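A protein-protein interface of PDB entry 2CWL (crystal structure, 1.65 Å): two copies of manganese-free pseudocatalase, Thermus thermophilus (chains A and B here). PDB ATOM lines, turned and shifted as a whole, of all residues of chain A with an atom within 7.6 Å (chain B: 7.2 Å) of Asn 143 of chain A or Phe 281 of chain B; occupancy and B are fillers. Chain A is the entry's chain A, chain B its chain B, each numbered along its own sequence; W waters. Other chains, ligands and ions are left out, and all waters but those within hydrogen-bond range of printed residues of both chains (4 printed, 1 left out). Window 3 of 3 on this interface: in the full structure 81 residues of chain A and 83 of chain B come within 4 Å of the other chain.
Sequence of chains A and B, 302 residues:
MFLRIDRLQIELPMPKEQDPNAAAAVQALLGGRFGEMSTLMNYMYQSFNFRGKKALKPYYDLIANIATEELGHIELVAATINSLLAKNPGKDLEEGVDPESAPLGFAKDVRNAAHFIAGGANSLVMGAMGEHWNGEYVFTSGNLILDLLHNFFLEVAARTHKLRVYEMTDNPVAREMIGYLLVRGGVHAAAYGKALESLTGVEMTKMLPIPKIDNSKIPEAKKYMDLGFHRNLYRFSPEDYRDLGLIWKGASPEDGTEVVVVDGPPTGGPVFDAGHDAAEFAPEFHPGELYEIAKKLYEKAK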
ATOM      1  N   GLN A  46      27.604 -12.071  12.227  1.00  0.00           N
ATOM      2  CA  GLN A  46      28.197 -13.368  12.523  1.00  0.00           C
ATOM      3  C   GLN A  46      29.075 -13.216  13.763  1.00  0.00           C
ATOM      4  O   GLN A  46      29.116 -14.105  14.614  1.00  0.00           O
ATOM      5  CB  GLN A  46      29.044 -13.863  11.349  1.00  0.00           C
ATOM      6  CG  GLN A  46      28.230 -14.342  10.154  1.00  0.00           C
ATOM      7  CD  GLN A  46      29.082 -14.532   8.917  1.00  0.00           C
ATOM      8  OE1 GLN A  46      30.310 -14.460   8.981  1.00  0.00           O
ATOM      9  NE2 GLN A  46      28.437 -14.775   7.782  1.00  0.00           N
ATOM     10  N   ASN A  49      26.775 -13.084  16.802  1.00  0.00           N
ATOM     11  CA  ASN A  49      26.192 -14.409  17.005  1.00  0.00           C
ATOM     12  C   ASN A  49      27.159 -15.575  17.168  1.00  0.00           C
ATOM     13  O   ASN A  49      26.730 -16.716  17.351  1.00  0.00           O
ATOM     14  CB  ASN A  49      25.241 -14.716  15.845  1.00  0.00           C
ATOM     15  CG  ASN A  49      24.185 -13.640  15.658  1.00  0.00           C
ATOM     16  OD1 ASN A  49      23.822 -12.946  16.606  1.00  0.00           O
ATOM     17  ND2 ASN A  49      23.676 -13.510  14.439  1.00  0.00           N
ATOM     18  N   PHE A  50      28.454 -15.291  17.122  1.00  0.00           N
ATOM     19  CA  PHE A  50      29.475 -16.330  17.222  1.00  0.00           C
ATOM     20  C   PHE A  50      29.405 -17.141  18.517  1.00  0.00           C
ATOM     21  O   PHE A  50      29.410 -16.579  19.613  1.00  0.00           O
ATOM     22  CB  PHE A  50      30.863 -15.691  17.095  1.00  0.00           C
ATOM     23  CG  PHE A  50      31.951 -16.656  16.704  1.00  0.00           C
ATOM     24  CD1 PHE A  50      32.394 -16.725  15.386  1.00  0.00           C
ATOM     25  CD2 PHE A  50      32.543 -17.484  17.655  1.00  0.00           C
ATOM     26  CE1 PHE A  50      33.417 -17.605  15.018  1.00  0.00           C
ATOM     27  CE2 PHE A  50      33.566 -18.366  17.300  1.00  0.00           C
ATOM     28  CZ  PHE A  50      34.004 -18.426  15.978  1.00  0.00           C
ATOM     29  N   ARG A  51      29.342 -18.463  18.383  1.00  0.00           N
ATOM     30  CA  ARG A  51      29.306 -19.348  19.544  1.00  0.00           C
ATOM     31  C   ARG A  51      30.690 -19.974  19.683  1.00  0.00           C
ATOM     32  O   ARG A  51      31.254 -20.476  18.709  1.00  0.00           O
ATOM     33  CB  ARG A  51      28.246 -20.436  19.355  1.00  0.00           C
ATOM     34  CG  ARG A  51      26.815 -19.921  19.429  1.00  0.00           C
ATOM     35  CD  ARG A  51      25.841 -20.975  18.922  1.00  0.00           C
ATOM     36  NE  ARG A  51      24.460 -20.498  18.872  1.00  0.00           N
ATOM     37  CZ  ARG A  51      23.569 -20.662  19.846  1.00  0.00           C
ATOM     38  NH1 ARG A  51      23.907 -21.292  20.962  1.00  0.00           N
ATOM     39  NH2 ARG A  51      22.328 -20.209  19.697  1.00  0.00           N
ATOM     40  N   ILE A  63      36.702 -13.094  12.026  1.00  0.00           N
ATOM     41  CA  ILE A  63      35.429 -12.506  11.623  1.00  0.00           C
ATOM     42  C   ILE A  63      35.161 -11.168  12.304  1.00  0.00           C
ATOM     43  O   ILE A  63      34.710 -10.216  11.663  1.00  0.00           O
ATOM     44  CB  ILE A  63      34.260 -13.477  11.905  1.00  0.00           C
ATOM     45  CG1 ILE A  63      34.458 -14.761  11.092  1.00  0.00           C
ATOM     46  CG2 ILE A  63      32.931 -12.823  11.537  1.00  0.00           C
ATOM     47  CD1 ILE A  63      33.381 -15.808  11.316  1.00  0.00           C
ATOM     48  N   PHE A 139      23.609 -13.509   5.997  1.00  0.00           N
ATOM     49  CA  PHE A 139      23.543 -14.933   6.298  1.00  0.00           C
ATOM     50  C   PHE A 139      24.310 -15.149   7.600  1.00  0.00           C
ATOM     51  O   PHE A 139      25.524 -14.946   7.654  1.00  0.00           O
ATOM     52  CB  PHE A 139      24.204 -15.753   5.187  1.00  0.00           C
ATOM     53  CG  PHE A 139      24.124 -17.240   5.405  1.00  0.00           C
ATOM     54  CD1 PHE A 139      22.991 -17.950   5.034  1.00  0.00           C
ATOM     55  CD2 PHE A 139      25.176 -17.927   6.006  1.00  0.00           C
ATOM     56  CE1 PHE A 139      22.902 -19.324   5.258  1.00  0.00           C
ATOM     57  CE2 PHE A 139      25.100 -19.300   6.235  1.00  0.00           C
ATOM     58  CZ  PHE A 139      23.961 -19.999   5.860  1.00  0.00           C
ATOM     59  N   THR A 140      23.599 -15.551   8.645  1.00  0.00           N
ATOM     60  CA  THR A 140      24.225 -15.795   9.938  1.00  0.00           C
ATOM     61  C   THR A 140      23.551 -17.039  10.526  1.00  0.00           C
ATOM     62  O   THR A 140      22.569 -16.966  11.268  1.00  0.00           O
ATOM     63  CB  THR A 140      24.097 -14.533  10.850  1.00  0.00           C
ATOM     64  OG1 THR A 140      24.696 -14.792  12.124  1.00  0.00           O
ATOM     65  CG2 THR A 140      22.647 -14.117  11.016  1.00  0.00           C
ATOM     66  N   SER A 141      24.107 -18.192  10.164  1.00  0.00           N
ATOM     67  CA  SER A 141      23.572 -19.492  10.561  1.00  0.00           C
ATOM     68  C   SER A 141      24.003 -20.028  11.913  1.00  0.00           C
ATOM     69  O   SER A 141      23.372 -20.939  12.443  1.00  0.00           O
ATOM     70  CB  SER A 141      23.942 -20.539   9.515  1.00  0.00           C
ATOM     71  OG  SER A 141      25.318 -20.874   9.626  1.00  0.00           O
ATOM     72  N   GLY A 142      25.083 -19.486  12.460  1.00  0.00           N
ATOM     73  CA  GLY A 142      25.570 -19.979  13.735  1.00  0.00           C
ATOM     74  C   GLY A 142      26.544 -21.127  13.540  1.00  0.00           C
ATOM     75  O   GLY A 142      27.282 -21.481  14.460  1.00  0.00           O
ATOM     76  N   ASN A 143      26.549 -21.721  12.347  1.00  0.00           N
ATOM     77  CA  ASN A 143      27.459 -22.827  12.043  1.00  0.00           C
ATOM     78  C   ASN A 143      28.707 -22.227  11.396  1.00  0.00           C
ATOM     79  O   ASN A 143      28.645 -21.641  10.314  1.00  0.00           O
ATOM     80  CB  ASN A 143      26.774 -23.835  11.109  1.00  0.00           C
ATOM     81  CG  ASN A 143      27.664 -25.012  10.758  1.00  0.00           C
ATOM     82  OD1 ASN A 143      28.502 -24.929   9.859  1.00  0.00           O
ATOM     83  ND2 ASN A 143      27.493 -26.118  11.475  1.00  0.00           N
ATOM     84  N   LEU A 144      29.845 -22.376  12.067  1.00  0.00           N
ATOM     85  CA  LEU A 144      31.101 -21.799  11.598  1.00  0.00           C
ATOM     86  C   LEU A 144      31.520 -22.122  10.166  1.00  0.00           C
ATOM     87  O   LEU A 144      31.783 -21.217   9.374  1.00  0.00           O
ATOM     88  CB  LEU A 144      32.236 -22.170  12.562  1.00  0.00           C
ATOM     89  CG  LEU A 144      33.616 -21.578  12.250  1.00  0.00           C
ATOM     90  CD1 LEU A 144      33.519 -20.062  12.119  1.00  0.00           C
ATOM     91  CD2 LEU A 144      34.594 -21.960  13.355  1.00  0.00           C
ATOM     92  N   ILE A 145      31.596 -23.402   9.829  1.00  0.00           N
ATOM     93  CA  ILE A 145      32.012 -23.781   8.486  1.00  0.00           C
ATOM     94  C   ILE A 145      31.033 -23.283   7.423  1.00  0.00           C
ATOM     95  O   ILE A 145      31.449 -22.783   6.377  1.00  0.00           O
ATOM     96  CB  ILE A 145      32.201 -25.311   8.387  1.00  0.00           C
ATOM     97  CG1 ILE A 145      33.401 -25.722   9.255  1.00  0.00           C
ATOM     98  CG2 ILE A 145      32.407 -25.727   6.938  1.00  0.00           C
ATOM     99  CD1 ILE A 145      33.588 -27.222   9.411  1.00  0.00           C
ATOM    100  N   LEU A 146      29.737 -23.411   7.691  1.00  0.00           N
ATOM    101  CA  LEU A 146      28.731 -22.950   6.739  1.00  0.00           C
ATOM    102  C   LEU A 146      28.861 -21.441   6.518  1.00  0.00           C
ATOM    103  O   LEU A 146      28.775 -20.968   5.384  1.00  0.00           O
ATOM    104  CB  LEU A 146      27.328 -23.295   7.247  1.00  0.00           C
ATOM    105  CG  LEU A 146      26.151 -22.948   6.328  1.00  0.00           C
ATOM    106  CD1 LEU A 146      26.305 -23.651   4.983  1.00  0.00           C
ATOM    107  CD2 LEU A 146      24.855 -23.370   7.003  1.00  0.00           C
ATOM    108  N   ASP A 147      29.068 -20.689   7.599  1.00  0.00           N
ATOM    109  CA  ASP A 147      29.226 -19.235   7.499  1.00  0.00           C
ATOM    110  C   ASP A 147      30.503 -18.879   6.736  1.00  0.00           C
ATOM    111  O   ASP A 147      30.510 -17.967   5.908  1.00  0.00           O
ATOM    112  CB  ASP A 147      29.301 -18.586   8.891  1.00  0.00           C
ATOM    113  CG  ASP A 147      27.947 -18.451   9.562  1.00  0.00           C
ATOM    114  OD1 ASP A 147      26.909 -18.703   8.914  1.00  0.00           O
ATOM    115  OD2 ASP A 147      27.929 -18.072  10.752  1.00  0.00           O
ATOM    116  N   LEU A 148      31.590 -19.591   7.025  1.00  0.00           N
ATOM    117  CA  LEU A 148      32.856 -19.326   6.352  1.00  0.00           C
ATOM    118  C   LEU A 148      32.768 -19.619   4.858  1.00  0.00           C
ATOM    119  O   LEU A 148      33.333 -18.887   4.044  1.00  0.00           O
ATOM    120  CB  LEU A 148      33.981 -20.148   6.988  1.00  0.00           C
ATOM    121  CG  LEU A 148      34.453 -19.638   8.351  1.00  0.00           C
ATOM    122  CD1 LEU A 148      35.430 -20.627   8.973  1.00  0.00           C
ATOM    123  CD2 LEU A 148      35.111 -18.274   8.176  1.00  0.00           C
ATOM    124  N   LEU A 149      32.060 -20.685   4.499  1.00  0.00           N
ATOM    125  CA  LEU A 149      31.897 -21.040   3.093  1.00  0.00           C
ATOM    126  C   LEU A 149      31.117 -19.913   2.424  1.00  0.00           C
ATOM    127  O   LEU A 149      31.460 -19.468   1.326  1.00  0.00           O
ATOM    128  CB  LEU A 149      31.136 -22.363   2.963  1.00  0.00           C
ATOM    129  CG  LEU A 149      30.772 -22.809   1.544  1.00  0.00           C
ATOM    130  CD1 LEU A 149      32.037 -22.966   0.700  1.00  0.00           C
ATOM    131  CD2 LEU A 149      30.006 -24.122   1.612  1.00  0.00           C
ATOM    132  N   VAL B  97      22.340 -34.827  22.001  1.00  0.00           N
ATOM    133  CA  VAL B  97      21.206 -34.270  21.271  1.00  0.00           C
ATOM    134  C   VAL B  97      20.960 -35.096  20.009  1.00  0.00           C
ATOM    135  O   VAL B  97      21.876 -35.341  19.226  1.00  0.00           O
ATOM    136  CB  VAL B  97      21.449 -32.793  20.893  1.00  0.00           C
ATOM    137  CG1 VAL B  97      20.286 -32.270  20.052  1.00  0.00           C
ATOM    138  CG2 VAL B  97      21.601 -31.959  22.158  1.00  0.00           C
ATOM    139  N   PRO B  99      18.448 -35.237  16.676  1.00  0.00           N
ATOM    140  CA  PRO B  99      17.425 -34.575  15.857  1.00  0.00           C
ATOM    141  C   PRO B  99      16.093 -35.322  15.792  1.00  0.00           C
ATOM    142  O   PRO B  99      15.033 -34.705  15.694  1.00  0.00           O
ATOM    143  CB  PRO B  99      18.094 -34.479  14.489  1.00  0.00           C
ATOM    144  CG  PRO B  99      19.537 -34.288  14.845  1.00  0.00           C
ATOM    145  CD  PRO B  99      19.733 -35.303  15.956  1.00  0.00           C
ATOM    146  N   LEU B 104      13.708 -29.117  18.626  1.00  0.00           N
ATOM    147  CA  LEU B 104      13.287 -27.745  18.347  1.00  0.00           C
ATOM    148  C   LEU B 104      11.766 -27.669  18.230  1.00  0.00           C
ATOM    149  O   LEU B 104      11.226 -26.715  17.677  1.00  0.00           O
ATOM    150  CB  LEU B 104      13.925 -27.243  17.048  1.00  0.00           C
ATOM    151  CG  LEU B 104      15.454 -27.160  17.013  1.00  0.00           C
ATOM    152  CD1 LEU B 104      15.909 -26.661  15.646  1.00  0.00           C
ATOM    153  CD2 LEU B 104      15.946 -26.227  18.113  1.00  0.00           C
ATOM    154  N   GLY B 120      20.825 -19.675  13.784  1.00  0.00           N
ATOM    155  CA  GLY B 120      21.102 -20.851  14.589  1.00  0.00           C
ATOM    156  C   GLY B 120      20.707 -20.442  15.993  1.00  0.00           C
ATOM    157  O   GLY B 120      21.529 -20.430  16.910  1.00  0.00           O
ATOM    158  N   ASN B 122      19.778 -17.443  16.823  1.00  0.00           N
ATOM    159  CA  ASN B 122      20.500 -16.194  17.040  1.00  0.00           C
ATOM    160  C   ASN B 122      19.810 -15.004  16.388  1.00  0.00           C
ATOM    161  O   ASN B 122      18.859 -15.167  15.622  1.00  0.00           O
ATOM    162  CB  ASN B 122      21.954 -16.300  16.545  1.00  0.00           C
ATOM    163  CG  ASN B 122      22.064 -16.701  15.080  1.00  0.00           C
ATOM    164  OD1 ASN B 122      21.551 -16.021  14.186  1.00  0.00           O
ATOM    165  ND2 ASN B 122      22.757 -17.804  14.828  1.00  0.00           N
ATOM    166  N   HIS B 276      27.098 -23.783  23.101  1.00  0.00           N
ATOM    167  CA  HIS B 276      26.749 -24.800  22.118  1.00  0.00           C
ATOM    168  C   HIS B 276      25.262 -25.151  22.100  1.00  0.00           C
ATOM    169  O   HIS B 276      24.654 -25.374  23.147  1.00  0.00           O
ATOM    170  CB  HIS B 276      27.555 -26.073  22.401  1.00  0.00           C
ATOM    171  CG  HIS B 276      27.295 -27.190  21.436  1.00  0.00           C
ATOM    172  ND1 HIS B 276      27.386 -28.517  21.798  1.00  0.00           N
ATOM    173  CD2 HIS B 276      26.975 -27.180  20.120  1.00  0.00           C
ATOM    174  CE1 HIS B 276      27.131 -29.277  20.747  1.00  0.00           C
ATOM    175  NE2 HIS B 276      26.880 -28.490  19.715  1.00  0.00           N
ATOM    176  N   ASP B 277      24.683 -25.176  20.902  1.00  0.00           N
ATOM    177  CA  ASP B 277      23.290 -25.572  20.711  1.00  0.00           C
ATOM    178  C   ASP B 277      23.384 -26.592  19.578  1.00  0.00           C
ATOM    179  O   ASP B 277      23.407 -26.232  18.400  1.00  0.00           O
ATOM    180  CB  ASP B 277      22.407 -24.387  20.284  1.00  0.00           C
ATOM    181  CG  ASP B 277      20.929 -24.765  20.193  1.00  0.00           C
ATOM    182  OD1 ASP B 277      20.633 -25.927  19.842  1.00  0.00           O
ATOM    183  OD2 ASP B 277      20.059 -23.906  20.457  1.00  0.00           O
ATOM    184  N   ALA B 278      23.465 -27.867  19.948  1.00  0.00           N
ATOM    185  CA  ALA B 278      23.598 -28.952  18.980  1.00  0.00           C
ATOM    186  C   ALA B 278      22.457 -29.038  17.970  1.00  0.00           C
ATOM    187  O   ALA B 278      22.690 -29.293  16.786  1.00  0.00           O
ATOM    188  CB  ALA B 278      23.743 -30.280  19.715  1.00  0.00           C
ATOM    189  N   ALA B 279      21.230 -28.831  18.435  1.00  0.00           N
ATOM    190  CA  ALA B 279      20.066 -28.891  17.556  1.00  0.00           C
ATOM    191  C   ALA B 279      20.171 -27.842  16.452  1.00  0.00           C
ATOM    192  O   ALA B 279      19.647 -28.028  15.354  1.00  0.00           O
ATOM    193  CB  ALA B 279      18.790 -28.684  18.359  1.00  0.00           C
ATOM    194  N   GLU B 280      20.852 -26.740  16.745  1.00  0.00           N
ATOM    195  CA  GLU B 280      21.026 -25.684  15.753  1.00  0.00           C
ATOM    196  C   GLU B 280      22.339 -25.861  14.991  1.00  0.00           C
ATOM    197  O   GLU B 280      22.652 -25.077  14.094  1.00  0.00           O
ATOM    198  CB  GLU B 280      20.997 -24.307  16.426  1.00  0.00           C
ATOM    199  CG  GLU B 280      19.615 -23.872  16.908  1.00  0.00           C
ATOM    200  CD  GLU B 280      18.624 -23.710  15.768  1.00  0.00           C
ATOM    201  OE1 GLU B 280      19.058 -23.676  14.597  1.00  0.00           O
ATOM    202  OE2 GLU B 280      17.410 -23.608  16.045  1.00  0.00           O
ATOM    203  N   PHE B 281      23.097 -26.897  15.349  1.00  0.00           N
ATOM    204  CA  PHE B 281      24.382 -27.186  14.708  1.00  0.00           C
ATOM    205  C   PHE B 281      25.282 -25.963  14.826  1.00  0.00           C
ATOM    206  O   PHE B 281      26.035 -25.631  13.909  1.00  0.00           O
ATOM    207  CB  PHE B 281      24.159 -27.538  13.230  1.00  0.00           C
ATOM    208  CG  PHE B 281      23.010 -28.479  13.008  1.00  0.00           C
ATOM    209  CD1 PHE B 281      23.052 -29.778  13.504  1.00  0.00           C
ATOM    210  CD2 PHE B 281      21.858 -28.050  12.352  1.00  0.00           C
ATOM    211  CE1 PHE B 281      21.962 -30.638  13.357  1.00  0.00           C
ATOM    212  CE2 PHE B 281      20.763 -28.901  12.200  1.00  0.00           C
ATOM    213  CZ  PHE B 281      20.815 -30.198  12.705  1.00  0.00           C
ATOM    214  N   ALA B 282      25.211 -25.302  15.976  1.00  0.00           N
ATOM    215  CA  ALA B 282      25.981 -24.088  16.210  1.00  0.00           C
ATOM    216  C   ALA B 282      26.804 -24.168  17.490  1.00  0.00           C
ATOM    217  O   ALA B 282      26.254 -24.366  18.573  1.00  0.00           O
ATOM    218  CB  ALA B 282      25.028 -22.900  16.280  1.00  0.00           C
ATOM    219  N   PRO B 283      28.132 -23.971  17.391  1.00  0.00           N
ATOM    220  CA  PRO B 283      28.918 -23.679  16.185  1.00  0.00           C
ATOM    221  C   PRO B 283      29.088 -24.869  15.240  1.00  0.00           C
ATOM    222  O   PRO B 283      29.550 -24.714  14.109  1.00  0.00           O
ATOM    223  CB  PRO B 283      30.243 -23.192  16.757  1.00  0.00           C
ATOM    224  CG  PRO B 283      30.391 -24.051  17.981  1.00  0.00           C
ATOM    225  CD  PRO B 283      29.001 -24.017  18.584  1.00  0.00           C
ATOM    226  N   GLU B 284      28.719 -26.051  15.723  1.00  0.00           N
ATOM    227  CA  GLU B 284      28.787 -27.287  14.950  1.00  0.00           C
ATOM    228  C   GLU B 284      27.880 -28.280  15.672  1.00  0.00           C
ATOM    229  O   GLU B 284      27.534 -28.062  16.835  1.00  0.00           O
ATOM    230  CB  GLU B 284      30.223 -27.820  14.907  1.00  0.00           C
ATOM    231  CG  GLU B 284      30.427 -29.032  13.997  1.00  0.00           C
ATOM    232  CD  GLU B 284      29.909 -28.798  12.590  1.00  0.00           C
ATOM    233  OE1 GLU B 284      28.691 -28.965  12.377  1.00  0.00           O
ATOM    234  OE2 GLU B 284      30.717 -28.435  11.702  1.00  0.00           O
ATOM    235  N   PHE B 285      27.482 -29.355  14.996  1.00  0.00           N
ATOM    236  CA  PHE B 285      26.621 -30.344  15.639  1.00  0.00           C
ATOM    237  C   PHE B 285      27.306 -30.778  16.932  1.00  0.00           C
ATOM    238  O   PHE B 285      26.705 -30.757  18.007  1.00  0.00           O
ATOM    239  CB  PHE B 285      26.392 -31.548  14.720  1.00  0.00           C
ATOM    240  CG  PHE B 285      25.536 -32.617  15.336  1.00  0.00           C
ATOM    241  CD1 PHE B 285      24.324 -32.293  15.938  1.00  0.00           C
ATOM    242  CD2 PHE B 285      25.946 -33.947  15.329  1.00  0.00           C
ATOM    243  CE1 PHE B 285      23.532 -33.273  16.532  1.00  0.00           C
ATOM    244  CE2 PHE B 285      25.162 -34.937  15.917  1.00  0.00           C
ATOM    245  CZ  PHE B 285      23.952 -34.598  16.521  1.00  0.00           C
ATOM    246  N   HIS B 286      28.569 -31.172  16.807  1.00  0.00           N
ATOM    247  CA  HIS B 286      29.392 -31.559  17.950  1.00  0.00           C
ATOM    248  C   HIS B 286      30.735 -30.903  17.636  1.00  0.00           C
ATOM    249  O   HIS B 286      31.496 -31.393  16.802  1.00  0.00           O
ATOM    250  CB  HIS B 286      29.545 -33.079  18.043  1.00  0.00           C
ATOM    251  CG  HIS B 286      30.207 -33.532  19.306  1.00  0.00           C
ATOM    252  ND1 HIS B 286      31.497 -33.175  19.637  1.00  0.00           N
ATOM    253  CD2 HIS B 286      29.746 -34.276  20.340  1.00  0.00           C
ATOM    254  CE1 HIS B 286      31.800 -33.677  20.821  1.00  0.00           C
ATOM    255  NE2 HIS B 286      30.755 -34.349  21.269  1.00  0.00           N
ATOM    256  N   LEU B 290      36.445 -29.484  16.172  1.00  0.00           N
ATOM    257  CA  LEU B 290      36.859 -28.131  15.821  1.00  0.00           C
ATOM    258  C   LEU B 290      37.607 -27.467  16.972  1.00  0.00           C
ATOM    259  O   LEU B 290      38.560 -26.718  16.749  1.00  0.00           O
ATOM    260  CB  LEU B 290      35.648 -27.285  15.416  1.00  0.00           C
ATOM    261  CG  LEU B 290      34.831 -27.821  14.237  1.00  0.00           C
ATOM    262  CD1 LEU B 290      33.864 -26.737  13.784  1.00  0.00           C
ATOM    263  CD2 LEU B 290      35.746 -28.224  13.085  1.00  0.00           C
HETATM  264  O   HOH W   1      23.458 -22.711  23.559  1.00  0.00           O
HETATM  265  O   HOH W   2      24.625 -18.472  16.798  1.00  0.00           O
HETATM  266  O   HOH W   3      29.564 -27.602   9.331  1.00  0.00           O
HETATM  267  O   HOH W   4      20.622 -21.545  21.588  1.00  0.00           O
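The side-chain amide nitrogen (ND2) of Asn 143 of chain A is in hydrogen-bond range of the backbone carbonyl oxygen (O) of Phe 281 of chain B (2.9 Å). O of Ser 141 of chain A lies close to N of Gly 120 of chain B (3.1 Å). ND2 of Asn 143 of chain A sits at hydrogen-bond distance from OE1 of Glu 284 of chain B (3.2 Å). The guanidinium group (NH2) of Arg 51 of chain A sits at hydrogen-bond distance from the backbone carbonyl oxygen (O) of Gly 120 of chain B (2.9 Å). ND2 of Asn 49 of chain A is in hydrogen-bond range of OD1 of Asn 122 of chain B (3.3 Å). The backbone carbonyl oxygen (O) of Thr 140 of chain A sits close to the side-chain amide oxygen (OD1) of Asn 122 of chain B (3.2 Å). The backbone carbonyl oxygen (O) of Pro 283 of chain B is in hydrogen-bond range of the backbone NH (N) of Leu 144 of chain A, at 3.1 Å.
OG1 of Thr 140 of chain A sits at hydrogen-bond distance from ND2 of Asn 49 of chain A (2.8 Å). NE2 of His 276 of chain B is in hydrogen-bond range of O of Glu 284 of chain B, at 3.0 Å. The backbone NH (N) of Asp 277 of chain B sits at hydrogen-bond distance from the backbone carbonyl oxygen (O) of Ala 282 of chain B, at 2.9 Å. OD1 of Asp 277 of chain B is in hydrogen-bond range of N of Glu 280 of chain B, 3.2 Å away. OD1 of Asp 147 of chain A lies within hydrogen-bond range of OG of Ser 141 of chain A (2.8 Å). The side-chain amide oxygen (OD1) of Asn 143 of chain A lies within hydrogen-bond range of the backbone NH (N) of Leu 146 of chain A, at 2.9 Å.
Among the printed residues, pairs that only touch across the chains: Arg 51 of chain A with Asp 277 of chain B (3.5 Å), Arg 51 of chain A with Ala 282 of chain B (3.4 Å), Arg 51 of chain A with Pro 283 of chain B (3.5 Å), Ser 141 of chain A with Asn 122 of chain B (3.9 Å), Gly 142 of chain A with Asn 122 of chain B (3.7 Å), Gly 142 of chain A with Ala 282 of chain B (3.2 Å), Gly 142 of chain A with Pro 283 of chain B (3.2 Å), Asn 143 of chain A with Pro 283 of chain B (3.5 Å) and Ile 145 of chain A with Glu 284 of chain B (3.9 Å).
Asn 143 of chain A touches just these residues of chain B: Phe 281 (2.9 Å), Pro 283 (3.5 Å) and Glu 284 (3.2 Å). Phe 281 of chain B touches just one residue of chain A: Asn 143 (2.9 Å). Of the printed residues of chain B, Gly 142 of chain A touches Asn 122, Ala 282 and Pro 283. Of the printed residues of chain A, Pro 283 of chain B touches Arg 51 (3.5 Å), Gly 142 (3.2 Å), Asn 143 (3.5 Å) and Leu 144 (3.1 Å). Of the printed residues of chain A, Glu 284 of chain B touches Asn 143 (3.2 Å) and Ile 145 (3.9 Å). Glu 280 of chain B touches none of the printed residues of chain A. His 276 of chain B touches none of the printed residues of chain A. The nearest printed residue of chain A that does not touch Pro 283 of chain B is Ile 145 of chain A (4.9 Å).
Of the 16 printed residues of chain A, 8 touch a printed residue of chain B. Hydrophobic or aromatic side chains of chain A within 4 Å of the printed part of chain B: Ile 145. Along chain B the printed residues that touch a printed residue of chain A span positions 120 to 284.
No position is printed for both chains. Of the 16 pairs that touch across the chains among the printed residues, none has its exchanged pair printed and touching as well.
Water W4 lies within hydrogen-bond range of OD2 of Asp 277 of chain B (2.7 Å) and NH2 of Arg 51 of chain A (2.9 Å). Water W3 lies within hydrogen-bond range of OE2 of Glu 284 of chain B (2.8 Å) and OD1 of Asn 143 of chain A (2.9 Å). Water W2 lies within hydrogen-bond range of ND2 of Asn 122 of chain B (2.8 Å), O of Asn 49 of chain A (2.8 Å) and NE of Arg 51 of chain A (2.9 Å). Water W1 lies within hydrogen-bond range of O of His 276 of chain B (2.9 Å) and NH1 of Arg 51 of chain A (3.0 Å).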
